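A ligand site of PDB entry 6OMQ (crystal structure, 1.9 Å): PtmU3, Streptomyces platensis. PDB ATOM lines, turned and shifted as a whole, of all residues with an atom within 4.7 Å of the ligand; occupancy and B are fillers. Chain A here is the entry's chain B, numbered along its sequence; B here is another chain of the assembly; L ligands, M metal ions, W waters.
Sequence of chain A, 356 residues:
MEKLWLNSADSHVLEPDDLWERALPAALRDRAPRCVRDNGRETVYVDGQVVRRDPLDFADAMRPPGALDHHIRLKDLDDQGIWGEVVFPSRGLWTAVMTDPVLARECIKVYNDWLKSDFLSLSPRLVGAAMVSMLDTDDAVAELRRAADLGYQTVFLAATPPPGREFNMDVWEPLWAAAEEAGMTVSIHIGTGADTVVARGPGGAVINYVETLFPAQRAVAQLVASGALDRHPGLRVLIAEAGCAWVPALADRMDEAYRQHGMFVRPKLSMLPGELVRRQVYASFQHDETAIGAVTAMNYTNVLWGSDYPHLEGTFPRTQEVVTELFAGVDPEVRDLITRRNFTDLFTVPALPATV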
ATOM      1  N   ARG A  52     -13.919 -19.769  36.793  1.00  0.00           N
ATOM      2  CA  ARG A  52     -14.812 -20.198  35.692  1.00  0.00           C
ATOM      3  C   ARG A  52     -16.168 -19.553  35.934  1.00  0.00           C
ATOM      4  O   ARG A  52     -16.615 -19.472  37.101  1.00  0.00           O
ATOM      5  CB  ARG A  52     -14.947 -21.721  35.596  1.00  0.00           C
ATOM      6  CG  ARG A  52     -15.723 -22.224  34.388  1.00  0.00           C
ATOM      7  CD  ARG A  52     -14.904 -22.384  33.109  1.00  0.00           C
ATOM      8  NE  ARG A  52     -15.771 -22.705  31.974  1.00  0.00           N
ATOM      9  CZ  ARG A  52     -15.378 -22.881  30.695  1.00  0.00           C
ATOM     10  NH1 ARG A  52     -14.102 -22.815  30.331  1.00  0.00           N
ATOM     11  NH2 ARG A  52     -16.304 -23.128  29.778  1.00  0.00           N
ATOM     12  N   ASP A  54     -19.936 -19.570  33.556  1.00  0.00           N
ATOM     13  CA  ASP A  54     -20.600 -20.280  32.439  1.00  0.00           C
ATOM     14  C   ASP A  54     -22.046 -19.831  32.475  1.00  0.00           C
ATOM     15  O   ASP A  54     -22.607 -19.609  33.554  1.00  0.00           O
ATOM     16  CB  ASP A  54     -20.471 -21.803  32.576  1.00  0.00           C
ATOM     17  CG  ASP A  54     -19.169 -22.434  32.116  1.00  0.00           C
ATOM     18  OD1 ASP A  54     -18.741 -22.136  30.995  1.00  0.00           O
ATOM     19  OD2 ASP A  54     -18.600 -23.268  32.869  1.00  0.00           O
ATOM     20  N   PHE A  58     -25.335 -23.792  29.436  1.00  0.00           N
ATOM     21  CA  PHE A  58     -24.190 -24.644  29.043  1.00  0.00           C
ATOM     22  C   PHE A  58     -23.843 -25.524  30.244  1.00  0.00           C
ATOM     23  O   PHE A  58     -23.711 -26.774  30.056  1.00  0.00           O
ATOM     24  CB  PHE A  58     -23.015 -23.788  28.520  1.00  0.00           C
ATOM     25  CG  PHE A  58     -21.745 -24.556  28.263  1.00  0.00           C
ATOM     26  CD1 PHE A  58     -21.726 -25.638  27.390  1.00  0.00           C
ATOM     27  CD2 PHE A  58     -20.551 -24.184  28.873  1.00  0.00           C
ATOM     28  CE1 PHE A  58     -20.539 -26.337  27.162  1.00  0.00           C
ATOM     29  CE2 PHE A  58     -19.374 -24.873  28.640  1.00  0.00           C
ATOM     30  CZ  PHE A  58     -19.362 -25.950  27.772  1.00  0.00           C
ATOM     31  N   MET A  62     -24.569 -29.985  30.328  1.00  0.00           N
ATOM     32  CA  MET A  62     -23.647 -31.075  30.733  1.00  0.00           C
ATOM     33  C   MET A  62     -24.187 -31.854  31.925  1.00  0.00           C
ATOM     34  O   MET A  62     -23.429 -32.684  32.467  1.00  0.00           O
ATOM     35  CB  MET A  62     -22.268 -30.499  31.081  1.00  0.00           C
ATOM     36  CG  MET A  62     -21.558 -29.917  29.882  1.00  0.00           C
ATOM     37  SD  MET A  62     -19.877 -29.314  30.352  1.00  0.00           S
ATOM     38  CE  MET A  62     -20.255 -27.614  30.785  1.00  0.00           C
ATOM     39  N   SER A  90     -15.266 -33.647  37.571  1.00  0.00           N
ATOM     40  CA  SER A  90     -15.746 -32.355  37.023  1.00  0.00           C
ATOM     41  C   SER A  90     -15.237 -31.233  37.940  1.00  0.00           C
ATOM     42  O   SER A  90     -14.177 -30.624  37.643  1.00  0.00           O
ATOM     43  CB  SER A  90     -17.222 -32.293  36.806  1.00  0.00           C
ATOM     44  OG  SER A  90     -17.642 -33.458  36.108  1.00  0.00           O
ATOM     45  N   LEU A  93     -11.520 -31.365  39.121  1.00  0.00           N
ATOM     46  CA  LEU A  93     -10.464 -30.939  38.152  1.00  0.00           C
ATOM     47  C   LEU A  93      -9.857 -29.623  38.629  1.00  0.00           C
ATOM     48  O   LEU A  93      -8.681 -29.370  38.342  1.00  0.00           O
ATOM     49  CB  LEU A  93     -11.102 -30.769  36.765  1.00  0.00           C
ATOM     50  CG  LEU A  93     -11.679 -32.041  36.144  1.00  0.00           C
ATOM     51  CD1 LEU A  93     -12.236 -31.727  34.761  1.00  0.00           C
ATOM     52  CD2 LEU A  93     -10.661 -33.152  36.044  1.00  0.00           C
ATOM     53  N   TRP A  94     -10.622 -28.801  39.360  1.00  0.00           N
ATOM     54  CA  TRP A  94     -10.130 -27.498  39.880  1.00  0.00           C
ATOM     55  C   TRP A  94      -9.016 -27.678  40.904  1.00  0.00           C
ATOM     56  O   TRP A  94      -8.311 -26.666  41.171  1.00  0.00           O
ATOM     57  CB  TRP A  94     -11.271 -26.659  40.445  1.00  0.00           C
ATOM     58  CG  TRP A  94     -12.289 -26.259  39.434  1.00  0.00           C
ATOM     59  CD1 TRP A  94     -13.619 -26.576  39.457  1.00  0.00           C
ATOM     60  CD2 TRP A  94     -12.053 -25.591  38.192  1.00  0.00           C
ATOM     61  NE1 TRP A  94     -14.239 -26.083  38.352  1.00  0.00           N
ATOM     62  CE2 TRP A  94     -13.308 -25.475  37.543  1.00  0.00           C
ATOM     63  CE3 TRP A  94     -10.921 -25.052  37.575  1.00  0.00           C
ATOM     64  CZ2 TRP A  94     -13.453 -24.861  36.307  1.00  0.00           C
ATOM     65  CZ3 TRP A  94     -11.063 -24.419  36.348  1.00  0.00           C
ATOM     66  CH2 TRP A  94     -12.323 -24.321  35.736  1.00  0.00           C
ATOM     67  N   ILE A 190      -7.274 -33.538  28.845  1.00  0.00           N
ATOM     68  CA  ILE A 190      -6.992 -32.178  28.334  1.00  0.00           C
ATOM     69  C   ILE A 190      -7.964 -31.170  28.940  1.00  0.00           C
ATOM     70  O   ILE A 190      -8.973 -31.572  29.650  1.00  0.00           O
ATOM     71  CB  ILE A 190      -6.925 -32.139  26.792  1.00  0.00           C
ATOM     72  CG1 ILE A 190      -8.208 -32.590  26.108  1.00  0.00           C
ATOM     73  CG2 ILE A 190      -5.742 -32.968  26.345  1.00  0.00           C
ATOM     74  CD1 ILE A 190      -9.429 -31.752  26.399  1.00  0.00           C
ATOM     75  N   GLY A 191      -7.661 -29.915  28.692  1.00  0.00           N
ATOM     76  CA  GLY A 191      -8.418 -28.757  29.183  1.00  0.00           C
ATOM     77  C   GLY A 191      -8.325 -28.627  30.700  1.00  0.00           C
ATOM     78  O   GLY A 191      -9.199 -27.920  31.266  1.00  0.00           O
ATOM     79  N   THR A 192      -7.299 -29.165  31.351  1.00  0.00           N
ATOM     80  CA  THR A 192      -7.137 -29.079  32.832  1.00  0.00           C
ATOM     81  C   THR A 192      -5.801 -28.392  33.185  1.00  0.00           C
ATOM     82  O   THR A 192      -4.858 -28.534  32.416  1.00  0.00           O
ATOM     83  CB  THR A 192      -7.240 -30.474  33.431  1.00  0.00           C
ATOM     84  OG1 THR A 192      -6.309 -31.356  32.815  1.00  0.00           O
ATOM     85  CG2 THR A 192      -8.613 -31.077  33.251  1.00  0.00           C
ATOM     86  N   THR A 196      -9.000 -22.318  29.841  1.00  0.00           N
ATOM     87  CA  THR A 196      -9.263 -22.897  28.491  1.00  0.00           C
ATOM     88  C   THR A 196      -9.759 -21.811  27.523  1.00  0.00           C
ATOM     89  O   THR A 196      -9.908 -22.103  26.315  1.00  0.00           O
ATOM     90  CB  THR A 196     -10.220 -24.079  28.642  1.00  0.00           C
ATOM     91  OG1 THR A 196     -11.450 -23.597  29.196  1.00  0.00           O
ATOM     92  CG2 THR A 196      -9.632 -25.192  29.497  1.00  0.00           C
ATOM     93  N   VAL A 197     -10.083 -20.620  28.032  1.00  0.00           N
ATOM     94  CA  VAL A 197     -10.530 -19.496  27.161  1.00  0.00           C
ATOM     95  C   VAL A 197      -9.279 -18.664  26.834  1.00  0.00           C
ATOM     96  O   VAL A 197      -8.917 -17.776  27.607  1.00  0.00           O
ATOM     97  CB  VAL A 197     -11.693 -18.692  27.772  1.00  0.00           C
ATOM     98  CG1 VAL A 197     -12.167 -17.600  26.813  1.00  0.00           C
ATOM     99  CG2 VAL A 197     -12.852 -19.605  28.175  1.00  0.00           C
ATOM    100  N   ALA A 199      -8.523 -17.747  23.255  1.00  0.00           N
ATOM    101  CA  ALA A 199      -8.901 -16.918  22.083  1.00  0.00           C
ATOM    102  C   ALA A 199     -10.237 -16.245  22.402  1.00  0.00           C
ATOM    103  O   ALA A 199     -11.099 -16.921  22.983  1.00  0.00           O
ATOM    104  CB  ALA A 199      -9.013 -17.796  20.863  1.00  0.00           C
ATOM    105  N   ARG A 200     -10.407 -14.971  22.022  1.00  0.00           N
ATOM    106  CA  ARG A 200     -11.704 -14.255  22.216  1.00  0.00           C
ATOM    107  C   ARG A 200     -12.191 -13.569  20.935  1.00  0.00           C
ATOM    108  O   ARG A 200     -13.357 -13.085  20.945  1.00  0.00           O
ATOM    109  CB  ARG A 200     -11.577 -13.248  23.358  1.00  0.00           C
ATOM    110  CG  ARG A 200     -11.616 -13.899  24.732  1.00  0.00           C
ATOM    111  CD  ARG A 200     -11.694 -12.898  25.862  1.00  0.00           C
ATOM    112  NE  ARG A 200     -11.816 -13.609  27.125  1.00  0.00           N
ATOM    113  CZ  ARG A 200     -10.809 -14.252  27.742  1.00  0.00           C
ATOM    114  NH1 ARG A 200      -9.602 -14.280  27.214  1.00  0.00           N
ATOM    115  NH2 ARG A 200     -11.025 -14.857  28.896  1.00  0.00           N
ATOM    116  N   GLY A 204     -13.582 -17.949  18.064  1.00  0.00           N
ATOM    117  CA  GLY A 204     -13.043 -18.200  19.412  1.00  0.00           C
ATOM    118  C   GLY A 204     -13.381 -19.587  19.901  1.00  0.00           C
ATOM    119  O   GLY A 204     -12.492 -20.217  20.427  1.00  0.00           O
ATOM    120  N   ALA A 205     -14.631 -20.033  19.788  1.00  0.00           N
ATOM    121  CA  ALA A 205     -15.077 -21.332  20.308  1.00  0.00           C
ATOM    122  C   ALA A 205     -14.271 -22.464  19.637  1.00  0.00           C
ATOM    123  O   ALA A 205     -13.754 -23.351  20.355  1.00  0.00           O
ATOM    124  CB  ALA A 205     -16.564 -21.498  20.099  1.00  0.00           C
ATOM    125  N   ASN A 208     -10.468 -22.229  20.711  1.00  0.00           N
ATOM    126  CA  ASN A 208     -10.187 -22.702  22.083  1.00  0.00           C
ATOM    127  C   ASN A 208     -10.226 -24.219  22.114  1.00  0.00           C
ATOM    128  O   ASN A 208      -9.401 -24.782  22.856  1.00  0.00           O
ATOM    129  CB  ASN A 208     -11.125 -22.080  23.120  1.00  0.00           C
ATOM    130  CG  ASN A 208     -10.801 -20.611  23.294  1.00  0.00           C
ATOM    131  OD1 ASN A 208      -9.622 -20.210  23.301  1.00  0.00           O
ATOM    132  ND2 ASN A 208     -11.848 -19.820  23.455  1.00  0.00           N
ATOM    133  N   TYR A 209     -11.112 -24.873  21.369  1.00  0.00           N
ATOM    134  CA  TYR A 209     -11.196 -26.353  21.394  1.00  0.00           C
ATOM    135  C   TYR A 209      -9.865 -26.882  20.817  1.00  0.00           C
ATOM    136  O   TYR A 209      -9.353 -27.841  21.344  1.00  0.00           O
ATOM    137  CB  TYR A 209     -12.491 -26.860  20.755  1.00  0.00           C
ATOM    138  CG  TYR A 209     -12.811 -28.305  21.076  1.00  0.00           C
ATOM    139  CD1 TYR A 209     -12.952 -28.751  22.378  1.00  0.00           C
ATOM    140  CD2 TYR A 209     -12.938 -29.257  20.062  1.00  0.00           C
ATOM    141  CE1 TYR A 209     -13.203 -30.076  22.683  1.00  0.00           C
ATOM    142  CE2 TYR A 209     -13.273 -30.578  20.355  1.00  0.00           C
ATOM    143  CZ  TYR A 209     -13.400 -31.013  21.669  1.00  0.00           C
ATOM    144  OH  TYR A 209     -13.614 -32.324  22.006  1.00  0.00           O
ATOM    145  N   THR A 212      -6.639 -26.544  23.380  1.00  0.00           N
ATOM    146  CA  THR A 212      -6.520 -27.543  24.487  1.00  0.00           C
ATOM    147  C   THR A 212      -5.604 -28.670  24.041  1.00  0.00           C
ATOM    148  O   THR A 212      -5.039 -29.366  24.916  1.00  0.00           O
ATOM    149  CB  THR A 212      -7.833 -28.195  24.946  1.00  0.00           C
ATOM    150  OG1 THR A 212      -8.299 -29.069  23.910  1.00  0.00           O
ATOM    151  CG2 THR A 212      -8.865 -27.160  25.307  1.00  0.00           C
ATOM    152  N   GLU A 241      -9.430 -37.270  25.539  1.00  0.00           N
ATOM    153  CA  GLU A 241     -10.286 -36.251  24.928  1.00  0.00           C
ATOM    154  C   GLU A 241      -9.462 -35.293  24.059  1.00  0.00           C
ATOM    155  O   GLU A 241      -9.886 -34.169  23.894  1.00  0.00           O
ATOM    156  CB  GLU A 241     -11.046 -35.440  26.002  1.00  0.00           C
ATOM    157  CG  GLU A 241     -12.347 -34.903  25.470  1.00  0.00           C
ATOM    158  CD  GLU A 241     -13.203 -34.069  26.407  1.00  0.00           C
ATOM    159  OE1 GLU A 241     -13.511 -34.509  27.558  1.00  0.00           O
ATOM    160  OE2 GLU A 241     -13.634 -32.986  25.909  1.00  0.00           O
ATOM    161  N   HIS A 311     -20.657 -34.485  28.289  1.00  0.00           N
ATOM    162  CA  HIS A 311     -20.252 -33.221  27.683  1.00  0.00           C
ATOM    163  C   HIS A 311     -20.869 -33.119  26.293  1.00  0.00           C
ATOM    164  O   HIS A 311     -21.109 -34.139  25.690  1.00  0.00           O
ATOM    165  CB  HIS A 311     -18.715 -33.125  27.679  1.00  0.00           C
ATOM    166  CG  HIS A 311     -18.138 -33.006  29.046  1.00  0.00           C
ATOM    167  ND1 HIS A 311     -16.781 -32.729  29.269  1.00  0.00           N
ATOM    168  CD2 HIS A 311     -18.742 -33.081  30.277  1.00  0.00           C
ATOM    169  CE1 HIS A 311     -16.579 -32.646  30.559  1.00  0.00           C
ATOM    170  NE2 HIS A 311     -17.769 -32.875  31.210  1.00  0.00           N
ATOM    171  N   GLU A 313     -19.299 -32.312  23.727  1.00  0.00           N
ATOM    172  CA  GLU A 313     -18.221 -32.761  22.794  1.00  0.00           C
ATOM    173  C   GLU A 313     -18.437 -34.250  22.530  1.00  0.00           C
ATOM    174  O   GLU A 313     -17.766 -34.783  21.641  1.00  0.00           O
ATOM    175  CB  GLU A 313     -16.799 -32.849  23.385  1.00  0.00           C
ATOM    176  CG  GLU A 313     -16.194 -31.718  24.103  1.00  0.00           C
ATOM    177  CD  GLU A 313     -16.715 -31.323  25.468  1.00  0.00           C
ATOM    178  OE1 GLU A 313     -16.200 -31.797  26.571  1.00  0.00           O
ATOM    179  OE2 GLU A 313     -17.638 -30.548  25.389  1.00  0.00           O
ATOM    180  N   HIS B 261     -20.509 -27.448  19.832  1.00  0.00           N
ATOM    181  CA  HIS B 261     -20.375 -26.206  20.631  1.00  0.00           C
ATOM    182  C   HIS B 261     -20.977 -25.066  19.815  1.00  0.00           C
ATOM    183  O   HIS B 261     -20.648 -23.908  20.101  1.00  0.00           O
ATOM    184  CB  HIS B 261     -18.906 -25.887  21.040  1.00  0.00           C
ATOM    185  CG  HIS B 261     -18.274 -26.809  22.020  1.00  0.00           C
ATOM    186  ND1 HIS B 261     -16.957 -26.644  22.425  1.00  0.00           N
ATOM    187  CD2 HIS B 261     -18.722 -27.917  22.653  1.00  0.00           C
ATOM    188  CE1 HIS B 261     -16.628 -27.601  23.266  1.00  0.00           C
ATOM    189  NE2 HIS B 261     -17.697 -28.400  23.431  1.00  0.00           N
ATOM    190  N   PHE B 264     -21.803 -21.411  20.928  1.00  0.00           N
ATOM    191  CA  PHE B 264     -20.696 -20.449  21.180  1.00  0.00           C
ATOM    192  C   PHE B 264     -20.053 -19.986  19.851  1.00  0.00           C
ATOM    193  O   PHE B 264     -19.214 -19.068  19.896  1.00  0.00           O
ATOM    194  CB  PHE B 264     -19.655 -21.091  22.107  1.00  0.00           C
ATOM    195  CG  PHE B 264     -20.085 -21.310  23.547  1.00  0.00           C
ATOM    196  CD1 PHE B 264     -20.038 -20.271  24.474  1.00  0.00           C
ATOM    197  CD2 PHE B 264     -20.485 -22.561  24.000  1.00  0.00           C
ATOM    198  CE1 PHE B 264     -20.385 -20.471  25.803  1.00  0.00           C
ATOM    199  CE2 PHE B 264     -20.838 -22.769  25.326  1.00  0.00           C
ATOM    200  CZ  PHE B 264     -20.796 -21.717  26.227  1.00  0.00           C
HETATM  201  C1  LIG L   1     -14.280 -28.649  33.279  1.00  0.00           C
HETATM  202  C2  LIG L   1     -12.420 -27.877  29.952  1.00  0.00           C
HETATM  203  C3  LIG L   1     -13.165 -28.428  27.508  1.00  0.00           C
HETATM  204  C4  LIG L   1     -12.706 -27.019  27.025  1.00  0.00           C
HETATM  205  C5  LIG L   1     -13.200 -23.847  26.008  1.00  0.00           C
HETATM  206  C6  LIG L   1     -15.508 -23.118  26.113  1.00  0.00           C
HETATM  207  C7  LIG L   1     -16.800 -22.227  24.143  1.00  0.00           C
HETATM  208  C8  LIG L   1     -15.490 -20.108  24.395  1.00  0.00           C
HETATM  209  O1  LIG L   1     -17.584 -13.886  24.047  1.00  0.00           O
HETATM  210  P1  LIG L   1     -16.131 -13.636  23.920  1.00  0.00           P
HETATM  211  O2  LIG L   1     -15.334 -13.405  25.153  1.00  0.00           O
HETATM  212  O3  LIG L   1     -15.619 -13.069  22.635  1.00  0.00           O
HETATM  213  O4  LIG L   1     -15.688 -15.213  23.609  1.00  0.00           O
HETATM  214  C9  LIG L   1     -15.905 -16.261  24.533  1.00  0.00           C
HETATM  215  C10 LIG L   1     -15.690 -17.601  23.800  1.00  0.00           C
HETATM  216  C11 LIG L   1     -16.915 -17.934  22.910  1.00  0.00           C
HETATM  217  C12 LIG L   1     -14.428 -17.529  22.911  1.00  0.00           C
HETATM  218  C13 LIG L   1     -15.533 -18.664  24.935  1.00  0.00           C
HETATM  219  O5  LIG L   1     -16.654 -18.543  25.859  1.00  0.00           O
HETATM  220  O6  LIG L   1     -14.489 -20.520  23.814  1.00  0.00           O
HETATM  221  N1  LIG L   1     -16.645 -20.828  24.571  1.00  0.00           N
HETATM  222  C14 LIG L   1     -16.922 -23.015  25.449  1.00  0.00           C
HETATM  223  O7  LIG L   1     -15.266 -22.578  27.202  1.00  0.00           O
HETATM  224  N2  LIG L   1     -14.531 -23.681  25.399  1.00  0.00           N
HETATM  225  C15 LIG L   1     -12.462 -24.902  25.163  1.00  0.00           C
HETATM  226  S1  LIG L   1     -13.285 -26.560  25.376  1.00  0.00           S
HETATM  227  O8  LIG L   1     -11.962 -26.296  27.689  1.00  0.00           O
HETATM  228  C16 LIG L   1     -11.970 -29.382  27.282  1.00  0.00           C
HETATM  229  C17 LIG L   1     -14.302 -28.986  26.662  1.00  0.00           C
HETATM  230  C18 LIG L   1     -15.666 -28.350  27.048  1.00  0.00           C
HETATM  231  C19 LIG L   1     -15.960 -28.578  28.510  1.00  0.00           C
HETATM  232  C20 LIG L   1     -14.938 -27.795  29.431  1.00  0.00           C
HETATM  233  C21 LIG L   1     -14.993 -26.255  29.218  1.00  0.00           C
HETATM  234  C22 LIG L   1     -15.212 -28.225  30.951  1.00  0.00           C
HETATM  235  C23 LIG L   1     -13.538 -28.433  29.092  1.00  0.00           C
HETATM  236  C24 LIG L   1     -12.652 -28.328  31.430  1.00  0.00           C
HETATM  237  O9  LIG L   1     -11.654 -27.671  32.309  1.00  0.00           O
HETATM  238  C25 LIG L   1     -14.015 -27.900  31.944  1.00  0.00           C
HETATM  239  C26 LIG L   1     -15.616 -28.057  33.695  1.00  0.00           C
HETATM  240  C27 LIG L   1     -15.834 -28.287  35.182  1.00  0.00           C
HETATM  241  O10 LIG L   1     -16.759 -28.585  32.853  1.00  0.00           O
HETATM  242  C28 LIG L   1     -16.583 -27.797  31.625  1.00  0.00           C
HETATM  243  C29 LIG L   1     -16.590 -26.393  32.206  1.00  0.00           C
HETATM  244  C30 LIG L   1     -15.451 -26.563  33.217  1.00  0.00           C
HETATM  245  C31 LIG L   1     -14.082 -26.478  32.491  1.00  0.00           C
HETATM  246 MN    MN M   1     -15.254 -32.976  27.448  1.00  0.00          MN
HETATM  247  O   HOH W   1     -19.800 -16.721  21.367  1.00  0.00           O
HETATM  248  O   HOH W   2     -13.788 -31.851  29.093  1.00  0.00           O
HETATM  249  O   HOH W   3     -10.558 -27.317  35.066  1.00  0.00           O
HETATM  250  O   HOH W   4     -16.337 -31.477  33.544  1.00  0.00           O
HETATM  251  O   HOH W   5     -17.201 -26.592  37.701  1.00  0.00           O
HETATM  252  O   HOH W   6     -16.248 -20.289  27.869  1.00  0.00           O
HETATM  253  O   HOH W   7     -17.658 -14.409  21.439  1.00  0.00           O
HETATM  254  O   HOH W   8     -14.894 -24.652  22.783  1.00  0.00           O
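An oxygen (O9) of the ligand is in hydrogen-bond range of the backbone carbonyl oxygen (O) of Gly 191, 2.7 Å away.
The guanidinium group of Arg 52 sits at hydrogen-bond distance from an oxygen (O7) of the ligand (2.8 Å).
ND2 of Asn 208 lies within hydrogen-bond range of O6 of the ligand (2.8 Å).
The side-chain hydroxyl (OG1) of Thr 196 lies close to an oxygen (O8) of the ligand (3.1 Å).
An oxygen (O3) of the ligand lies close to the backbone carbonyl oxygen of Arg 200.
OD2 of Asp 54 touches C29 of the ligand (3.8 Å).
CE of Met 62 touches C28 of the ligand, at 3.8 Å.
Ser 90 touches the ligand.
CD1 of Leu 93 touches C1 of the ligand, 3.98 Å away.
Ile 190 touches the ligand (CD1 to C16, 3.6 Å).
Val 197 touches the ligand.
Ala 199 touches the ligand.
C of Gly 204 touches C12 of the ligand, at 3.8 Å.
Ala 205 touches the ligand (CA to O6, 3.6 Å).
CD1 of Tyr 209 touches S1 of the ligand (3.7 Å).
OE2 of Glu 313 touches C18 of the ligand (3.4 Å).
CE1 of His 261 of chain B touches C18 of the ligand, at 3.97 Å.
Phe 264 of chain B touches the ligand (CD1 to N1, 3.4 Å).
Hydrophobic or aromatic side chains that line the ligand: Met 62, Leu 93, Ile 190, Val 197, Tyr 209, His 261 of chain B and Phe 264 of chain B.
Within 4 Å of the ligand: Arg 52, Asp 54, Met 62, Ser 90, Leu 93, Ile 190, Gly 191, Thr 196, Val 197, Ala 199, Arg 200, Gly 204, Ala 205, Asn 208, Tyr 209, Glu 313, His 261 of chain B and Phe 264 of chain B.
Water W6 lies within hydrogen-bond range of O7 of the ligand and NH2 of Arg 52.
Water W8 lies within hydrogen-bond range of N2 of the ligand, ND1 of His 261 of chain B and O of Ala 205.
Water W4 lies within hydrogen-bond range of an oxygen (O10) of the ligand (3.0 Å), a ring nitrogen (NE2) of His 311 (3.1 Å) and the side-chain hydroxyl of Ser 90 (3.5 Å).
OG1 of Thr 196 sits at hydrogen-bond distance from NH1 of Arg 52 (3.0 Å).
ND2 of Asn 208 is in hydrogen-bond range of O of Gly 204 (3.1 Å).
OD1 of Asn 208 is in hydrogen-bond range of N of Ala 199, at 2.7 Å.
The side-chain carboxylate (OE2) of Glu 313 sits at hydrogen-bond distance from a ring nitrogen (NE2) of His 261 of chain B (2.9 Å).
The guanidinium group (NH2) of Arg 52 lies within salt-bridge range of the side-chain carboxylate (OD1) of Asp 54.
The backbone carbonyl oxygen (O) of Tyr 209 is in hydrogen-bond range of the side-chain hydroxyl (OG1) of Thr 212 (3.0 Å).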
